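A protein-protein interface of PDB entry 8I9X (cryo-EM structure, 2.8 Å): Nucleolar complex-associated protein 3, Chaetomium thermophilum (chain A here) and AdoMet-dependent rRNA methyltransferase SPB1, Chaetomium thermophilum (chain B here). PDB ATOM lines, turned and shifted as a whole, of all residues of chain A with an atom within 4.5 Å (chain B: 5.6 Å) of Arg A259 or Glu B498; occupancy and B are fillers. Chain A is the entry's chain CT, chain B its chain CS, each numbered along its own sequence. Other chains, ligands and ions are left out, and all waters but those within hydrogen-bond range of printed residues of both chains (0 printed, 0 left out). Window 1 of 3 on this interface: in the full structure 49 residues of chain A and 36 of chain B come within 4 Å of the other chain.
Of the 6 printed residues of chain B, 3 touch a printed residue of chain A.
Printed residues of chain B that touch a printed residue of chain A: Glu B498, Val B499 and Asp B501.
Among the printed residues, 5 pairs touch across the chains.
Among the printed residues, Asp or Glu carboxylates within 4 Å of a Lys or Arg side-chain nitrogen of the other chain: Arg A259 with Glu B498.
The backbone carbonyl oxygen (O) of Pro A254 lies close to the guanidinium group (NH1) of Arg A259, at 3.3 Å.
The guanidinium group of Arg A183 is in hydrogen-bond range of the backbone carbonyl oxygen of His A255 (2.6 Å).
The backbone carbonyl oxygen of Phe A256 sits at hydrogen-bond distance from the guanidinium group of Arg A183.
The side-chain carboxylate (OE1) of Glu A301 is in salt-bridge range of the guanidinium group (NE) of Arg A259.
Of chain B, only Glu B498 (3.6 Å) comes within 4 Å of Arg A259.
Of the printed residues of chain A, Glu B498 touches Arg A259 and Asn A297.
Of the printed residues of chain A, Asp B501 touches Phe A258.
Printed residues of chain B within 4 Å of Asn A297: Glu B498.
Printed residues of chain B within 4 Å of Phe A258: Asp B501.
Printed residues of chain B within 4 Å of Asn A257: Val B499.
Printed residues of chain A within 4 Å of Val B499: Arg A183 (2.5 Å) and Asn A257 (3.9 Å).
The nearest residue of chain B that does not touch Arg A259 is Asp B501 (4.7 Å).
Asn A257 touches Val B499.
N of Phe A258 sits at hydrogen-bond distance from OD2 of Asp B501, 3.4 Å away.
The side-chain carboxylate (OE1) of Glu B498 lies within salt-bridge range of the guanidinium group (NH2) of Arg A259 (3.6 Å).
ND2 of Asn A297 sits at hydrogen-bond distance from OE1 of Glu B498 (2.9 Å).
The backbone carbonyl oxygen of Val B499 is in hydrogen-bond range of the guanidinium group of Arg A183 (2.5 Å).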
ATOM      1  N   ARG A 183      -5.712   3.862  32.497  1.00  0.00           N
ATOM      2  CA  ARG A 183      -4.362   4.048  32.999  1.00  0.00           C
ATOM      3  C   ARG A 183      -4.406   4.486  34.458  1.00  0.00           C
ATOM      4  O   ARG A 183      -5.442   4.914  34.971  1.00  0.00           O
ATOM      5  CB  ARG A 183      -3.611   5.080  32.159  1.00  0.00           C
ATOM      6  CG  ARG A 183      -3.319   4.634  30.740  1.00  0.00           C
ATOM      7  CD  ARG A 183      -2.581   5.715  29.974  1.00  0.00           C
ATOM      8  NE  ARG A 183      -2.141   5.261  28.662  1.00  0.00           N
ATOM      9  CZ  ARG A 183      -1.393   5.978  27.836  1.00  0.00           C
ATOM     10  NH1 ARG A 183      -0.981   7.193  28.156  1.00  0.00           N
ATOM     11  NH2 ARG A 183      -1.048   5.463  26.660  1.00  0.00           N
ATOM     12  N   PRO A 254      -4.309  -1.018  23.681  1.00  0.00           N
ATOM     13  CA  PRO A 254      -3.663   0.217  23.218  1.00  0.00           C
ATOM     14  C   PRO A 254      -3.731   1.325  24.256  1.00  0.00           C
ATOM     15  O   PRO A 254      -2.821   2.154  24.354  1.00  0.00           O
ATOM     16  CB  PRO A 254      -4.458   0.587  21.956  1.00  0.00           C
ATOM     17  CG  PRO A 254      -5.374  -0.573  21.683  1.00  0.00           C
ATOM     18  CD  PRO A 254      -5.579  -1.266  22.982  1.00  0.00           C
ATOM     19  N   HIS A 255      -4.811   1.342  25.035  1.00  0.00           N
ATOM     20  CA  HIS A 255      -5.081   2.414  25.986  1.00  0.00           C
ATOM     21  C   HIS A 255      -4.057   2.479  27.112  1.00  0.00           C
ATOM     22  O   HIS A 255      -3.806   3.554  27.665  1.00  0.00           O
ATOM     23  CB  HIS A 255      -6.479   2.248  26.576  1.00  0.00           C
ATOM     24  CG  HIS A 255      -6.777   0.853  27.026  1.00  0.00           C
ATOM     25  ND1 HIS A 255      -6.318   0.343  28.220  1.00  0.00           N
ATOM     26  CD2 HIS A 255      -7.481  -0.143  26.438  1.00  0.00           C
ATOM     27  CE1 HIS A 255      -6.728  -0.906  28.350  1.00  0.00           C
ATOM     28  NE2 HIS A 255      -7.437  -1.225  27.283  1.00  0.00           N
ATOM     29  N   PHE A 256      -3.462   1.342  27.462  1.00  0.00           N
ATOM     30  CA  PHE A 256      -2.639   1.280  28.658  1.00  0.00           C
ATOM     31  C   PHE A 256      -1.273   1.924  28.412  1.00  0.00           C
ATOM     32  O   PHE A 256      -0.940   2.361  27.308  1.00  0.00           O
ATOM     33  CB  PHE A 256      -2.479  -0.168  29.119  1.00  0.00           C
ATOM     34  CG  PHE A 256      -2.064  -0.304  30.557  1.00  0.00           C
ATOM     35  CD1 PHE A 256      -2.744   0.373  31.553  1.00  0.00           C
ATOM     36  CD2 PHE A 256      -0.993  -1.105  30.910  1.00  0.00           C
ATOM     37  CE1 PHE A 256      -2.366   0.253  32.874  1.00  0.00           C
ATOM     38  CE2 PHE A 256      -0.610  -1.228  32.230  1.00  0.00           C
ATOM     39  CZ  PHE A 256      -1.297  -0.547  33.213  1.00  0.00           C
ATOM     40  N   ASN A 257      -0.476   1.973  29.477  1.00  0.00           N
ATOM     41  CA  ASN A 257       0.780   2.703  29.491  1.00  0.00           C
ATOM     42  C   ASN A 257       1.815   2.046  28.578  1.00  0.00           C
ATOM     43  O   ASN A 257       1.711   0.875  28.203  1.00  0.00           O
ATOM     44  CB  ASN A 257       1.325   2.782  30.914  1.00  0.00           C
ATOM     45  CG  ASN A 257       0.499   3.680  31.804  1.00  0.00           C
ATOM     46  OD1 ASN A 257       0.069   4.754  31.391  1.00  0.00           O
ATOM     47  ND2 ASN A 257       0.269   3.242  33.034  1.00  0.00           N
ATOM     48  N   PHE A 258       2.824   2.841  28.215  1.00  0.00           N
ATOM     49  CA  PHE A 258       4.017   2.373  27.505  1.00  0.00           C
ATOM     50  C   PHE A 258       3.663   1.810  26.126  1.00  0.00           C
ATOM     51  O   PHE A 258       4.417   1.035  25.513  1.00  0.00           O
ATOM     52  CB  PHE A 258       4.792   1.378  28.365  1.00  0.00           C
ATOM     53  CG  PHE A 258       5.384   2.008  29.595  1.00  0.00           C
ATOM     54  CD1 PHE A 258       6.566   2.726  29.526  1.00  0.00           C
ATOM     55  CD2 PHE A 258       4.736   1.912  30.817  1.00  0.00           C
ATOM     56  CE1 PHE A 258       7.097   3.326  30.653  1.00  0.00           C
ATOM     57  CE2 PHE A 258       5.266   2.502  31.949  1.00  0.00           C
ATOM     58  CZ  PHE A 258       6.448   3.207  31.868  1.00  0.00           C
ATOM     59  N   ARG A 259       2.505   2.247  25.625  1.00  0.00           N
ATOM     60  CA  ARG A 259       2.210   2.144  24.204  1.00  0.00           C
ATOM     61  C   ARG A 259       3.363   2.686  23.377  1.00  0.00           C
ATOM     62  O   ARG A 259       3.601   2.226  22.256  1.00  0.00           O
ATOM     63  CB  ARG A 259       0.925   2.907  23.892  1.00  0.00           C
ATOM     64  CG  ARG A 259       0.454   2.809  22.458  1.00  0.00           C
ATOM     65  CD  ARG A 259      -0.828   3.597  22.277  1.00  0.00           C
ATOM     66  NE  ARG A 259      -0.709   4.947  22.813  1.00  0.00           N
ATOM     67  CZ  ARG A 259      -1.730   5.674  23.245  1.00  0.00           C
ATOM     68  NH1 ARG A 259      -2.969   5.213  23.211  1.00  0.00           N
ATOM     69  NH2 ARG A 259      -1.502   6.893  23.724  1.00  0.00           N
ATOM     70  N   GLY A 260       4.095   3.660  23.919  1.00  0.00           N
ATOM     71  CA  GLY A 260       5.276   4.153  23.239  1.00  0.00           C
ATOM     72  C   GLY A 260       6.320   3.083  23.004  1.00  0.00           C
ATOM     73  O   GLY A 260       6.812   2.935  21.887  1.00  0.00           O
ATOM     74  N   ASP A 261       6.657   2.308  24.038  1.00  0.00           N
ATOM     75  CA  ASP A 261       7.631   1.235  23.862  1.00  0.00           C
ATOM     76  C   ASP A 261       7.102   0.158  22.924  1.00  0.00           C
ATOM     77  O   ASP A 261       7.836  -0.341  22.056  1.00  0.00           O
ATOM     78  CB  ASP A 261       7.999   0.628  25.215  1.00  0.00           C
ATOM     79  CG  ASP A 261       9.067   1.421  25.936  1.00  0.00           C
ATOM     80  OD1 ASP A 261       9.416   2.521  25.461  1.00  0.00           O
ATOM     81  OD2 ASP A 261       9.564   0.939  26.976  1.00  0.00           O
ATOM     82  N   LEU A 262       5.830  -0.209  23.082  1.00  0.00           N
ATOM     83  CA  LEU A 262       5.249  -1.233  22.215  1.00  0.00           C
ATOM     84  C   LEU A 262       5.316  -0.820  20.743  1.00  0.00           C
ATOM     85  O   LEU A 262       5.835  -1.560  19.888  1.00  0.00           O
ATOM     86  CB  LEU A 262       3.812  -1.499  22.662  1.00  0.00           C
ATOM     87  CG  LEU A 262       3.058  -2.765  22.274  1.00  0.00           C
ATOM     88  CD1 LEU A 262       3.609  -3.969  22.995  1.00  0.00           C
ATOM     89  CD2 LEU A 262       1.602  -2.570  22.652  1.00  0.00           C
ATOM     90  N   LEU A 263       4.830   0.382  20.434  1.00  0.00           N
ATOM     91  CA  LEU A 263       4.861   0.874  19.068  1.00  0.00           C
ATOM     92  C   LEU A 263       6.280   1.126  18.582  1.00  0.00           C
ATOM     93  O   LEU A 263       6.537   1.020  17.380  1.00  0.00           O
ATOM     94  CB  LEU A 263       4.031   2.151  18.964  1.00  0.00           C
ATOM     95  CG  LEU A 263       2.519   1.942  18.998  1.00  0.00           C
ATOM     96  CD1 LEU A 263       1.789   3.272  18.922  1.00  0.00           C
ATOM     97  CD2 LEU A 263       2.082   1.019  17.879  1.00  0.00           C
ATOM     98  N   ASN A 297      -5.604   8.822  20.021  1.00  0.00           N
ATOM     99  CA  ASN A 297      -4.289   9.066  20.605  1.00  0.00           C
ATOM    100  C   ASN A 297      -3.280   8.007  20.177  1.00  0.00           C
ATOM    101  O   ASN A 297      -2.128   8.330  19.852  1.00  0.00           O
ATOM    102  CB  ASN A 297      -4.405   9.124  22.126  1.00  0.00           C
ATOM    103  CG  ASN A 297      -5.139  10.361  22.606  1.00  0.00           C
ATOM    104  OD1 ASN A 297      -4.929  11.460  22.093  1.00  0.00           O
ATOM    105  ND2 ASN A 297      -6.009  10.186  23.593  1.00  0.00           N
ATOM    106  N   ALA A 298      -3.693   6.739  20.168  1.00  0.00           N
ATOM    107  CA  ALA A 298      -2.811   5.672  19.707  1.00  0.00           C
ATOM    108  C   ALA A 298      -2.428   5.878  18.249  1.00  0.00           C
ATOM    109  O   ALA A 298      -1.260   5.714  17.872  1.00  0.00           O
ATOM    110  CB  ALA A 298      -3.485   4.316  19.902  1.00  0.00           C
ATOM    111  N   GLU A 301       0.145   8.750  17.999  1.00  0.00           N
ATOM    112  CA  GLU A 301       1.493   8.393  18.428  1.00  0.00           C
ATOM    113  C   GLU A 301       2.154   7.448  17.430  1.00  0.00           C
ATOM    114  O   GLU A 301       3.350   7.581  17.133  1.00  0.00           O
ATOM    115  CB  GLU A 301       1.441   7.791  19.830  1.00  0.00           C
ATOM    116  CG  GLU A 301       2.790   7.455  20.429  1.00  0.00           C
ATOM    117  CD  GLU A 301       2.673   6.919  21.840  1.00  0.00           C
ATOM    118  OE1 GLU A 301       1.535   6.790  22.338  1.00  0.00           O
ATOM    119  OE2 GLU A 301       3.721   6.656  22.463  1.00  0.00           O
ATOM    120  N   ARG B 496     -11.362  12.401  29.945  1.00  0.00           N
ATOM    121  CA  ARG B 496     -10.895  11.880  28.667  1.00  0.00           C
ATOM    122  C   ARG B 496      -9.398  12.060  28.443  1.00  0.00           C
ATOM    123  O   ARG B 496      -8.863  11.494  27.483  1.00  0.00           O
ATOM    124  CB  ARG B 496     -11.665  12.529  27.516  1.00  0.00           C
ATOM    125  CG  ARG B 496     -13.129  12.144  27.484  1.00  0.00           C
ATOM    126  CD  ARG B 496     -13.843  12.838  26.353  1.00  0.00           C
ATOM    127  NE  ARG B 496     -13.334  12.415  25.056  1.00  0.00           N
ATOM    128  CZ  ARG B 496     -13.784  11.362  24.386  1.00  0.00           C
ATOM    129  NH1 ARG B 496     -14.750  10.598  24.868  1.00  0.00           N
ATOM    130  NH2 ARG B 496     -13.257  11.075  23.200  1.00  0.00           N
ATOM    131  N   GLN B 497      -8.716  12.826  29.286  1.00  0.00           N
ATOM    132  CA  GLN B 497      -7.292  13.064  29.101  1.00  0.00           C
ATOM    133  C   GLN B 497      -6.478  11.865  29.569  1.00  0.00           C
ATOM    134  O   GLN B 497      -6.671  11.357  30.678  1.00  0.00           O
ATOM    135  CB  GLN B 497      -6.873  14.328  29.855  1.00  0.00           C
ATOM    136  CG  GLN B 497      -5.451  14.796  29.589  1.00  0.00           C
ATOM    137  CD  GLN B 497      -4.429  14.117  30.478  1.00  0.00           C
ATOM    138  OE1 GLN B 497      -4.732  13.727  31.606  1.00  0.00           O
ATOM    139  NE2 GLN B 497      -3.209  13.975  29.976  1.00  0.00           N
ATOM    140  N   GLU B 498      -5.561  11.414  28.719  1.00  0.00           N
ATOM    141  CA  GLU B 498      -4.705  10.281  29.036  1.00  0.00           C
ATOM    142  C   GLU B 498      -3.383  10.751  29.627  1.00  0.00           C
ATOM    143  O   GLU B 498      -2.842  11.792  29.247  1.00  0.00           O
ATOM    144  CB  GLU B 498      -4.440   9.425  27.797  1.00  0.00           C
ATOM    145  CG  GLU B 498      -5.682   8.794  27.190  1.00  0.00           C
ATOM    146  CD  GLU B 498      -5.390   8.087  25.882  1.00  0.00           C
ATOM    147  OE1 GLU B 498      -4.368   8.415  25.243  1.00  0.00           O
ATOM    148  OE2 GLU B 498      -6.181   7.202  25.492  1.00  0.00           O
ATOM    149  N   VAL B 499      -2.861   9.958  30.561  1.00  0.00           N
ATOM    150  CA  VAL B 499      -1.649  10.337  31.273  1.00  0.00           C
ATOM    151  C   VAL B 499      -0.424  10.022  30.423  1.00  0.00           C
ATOM    152  O   VAL B 499      -0.482   9.239  29.465  1.00  0.00           O
ATOM    153  CB  VAL B 499      -1.586   9.620  32.632  1.00  0.00           C
ATOM    154  CG1 VAL B 499      -2.780  10.019  33.478  1.00  0.00           C
ATOM    155  CG2 VAL B 499      -1.534   8.117  32.441  1.00  0.00           C
ATOM    156  N   ASP B 500       0.701  10.644  30.773  1.00  0.00           N
ATOM    157  CA  ASP B 500       1.913  10.551  29.970  1.00  0.00           C
ATOM    158  C   ASP B 500       2.898   9.573  30.606  1.00  0.00           C
ATOM    159  O   ASP B 500       2.627   9.031  31.683  1.00  0.00           O
ATOM    160  CB  ASP B 500       2.519  11.949  29.809  1.00  0.00           C
ATOM    161  CG  ASP B 500       3.702  11.976  28.867  1.00  0.00           C
ATOM    162  OD1 ASP B 500       3.491  11.881  27.640  1.00  0.00           O
ATOM    163  OD2 ASP B 500       4.841  12.092  29.356  1.00  0.00           O
ATOM    164  N   ASP B 501       4.040   9.335  29.956  1.00  0.00           N
ATOM    165  CA  ASP B 501       5.018   8.387  30.478  1.00  0.00           C
ATOM    166  C   ASP B 501       6.247   9.045  31.090  1.00  0.00           C
ATOM    167  O   ASP B 501       6.998   8.359  31.791  1.00  0.00           O
ATOM    168  CB  ASP B 501       5.451   7.415  29.368  1.00  0.00           C
ATOM    169  CG  ASP B 501       4.284   6.646  28.777  1.00  0.00           C
ATOM    170  OD1 ASP B 501       3.137   6.874  29.212  1.00  0.00           O
ATOM    171  OD2 ASP B 501       4.516   5.809  27.879  1.00  0.00           O
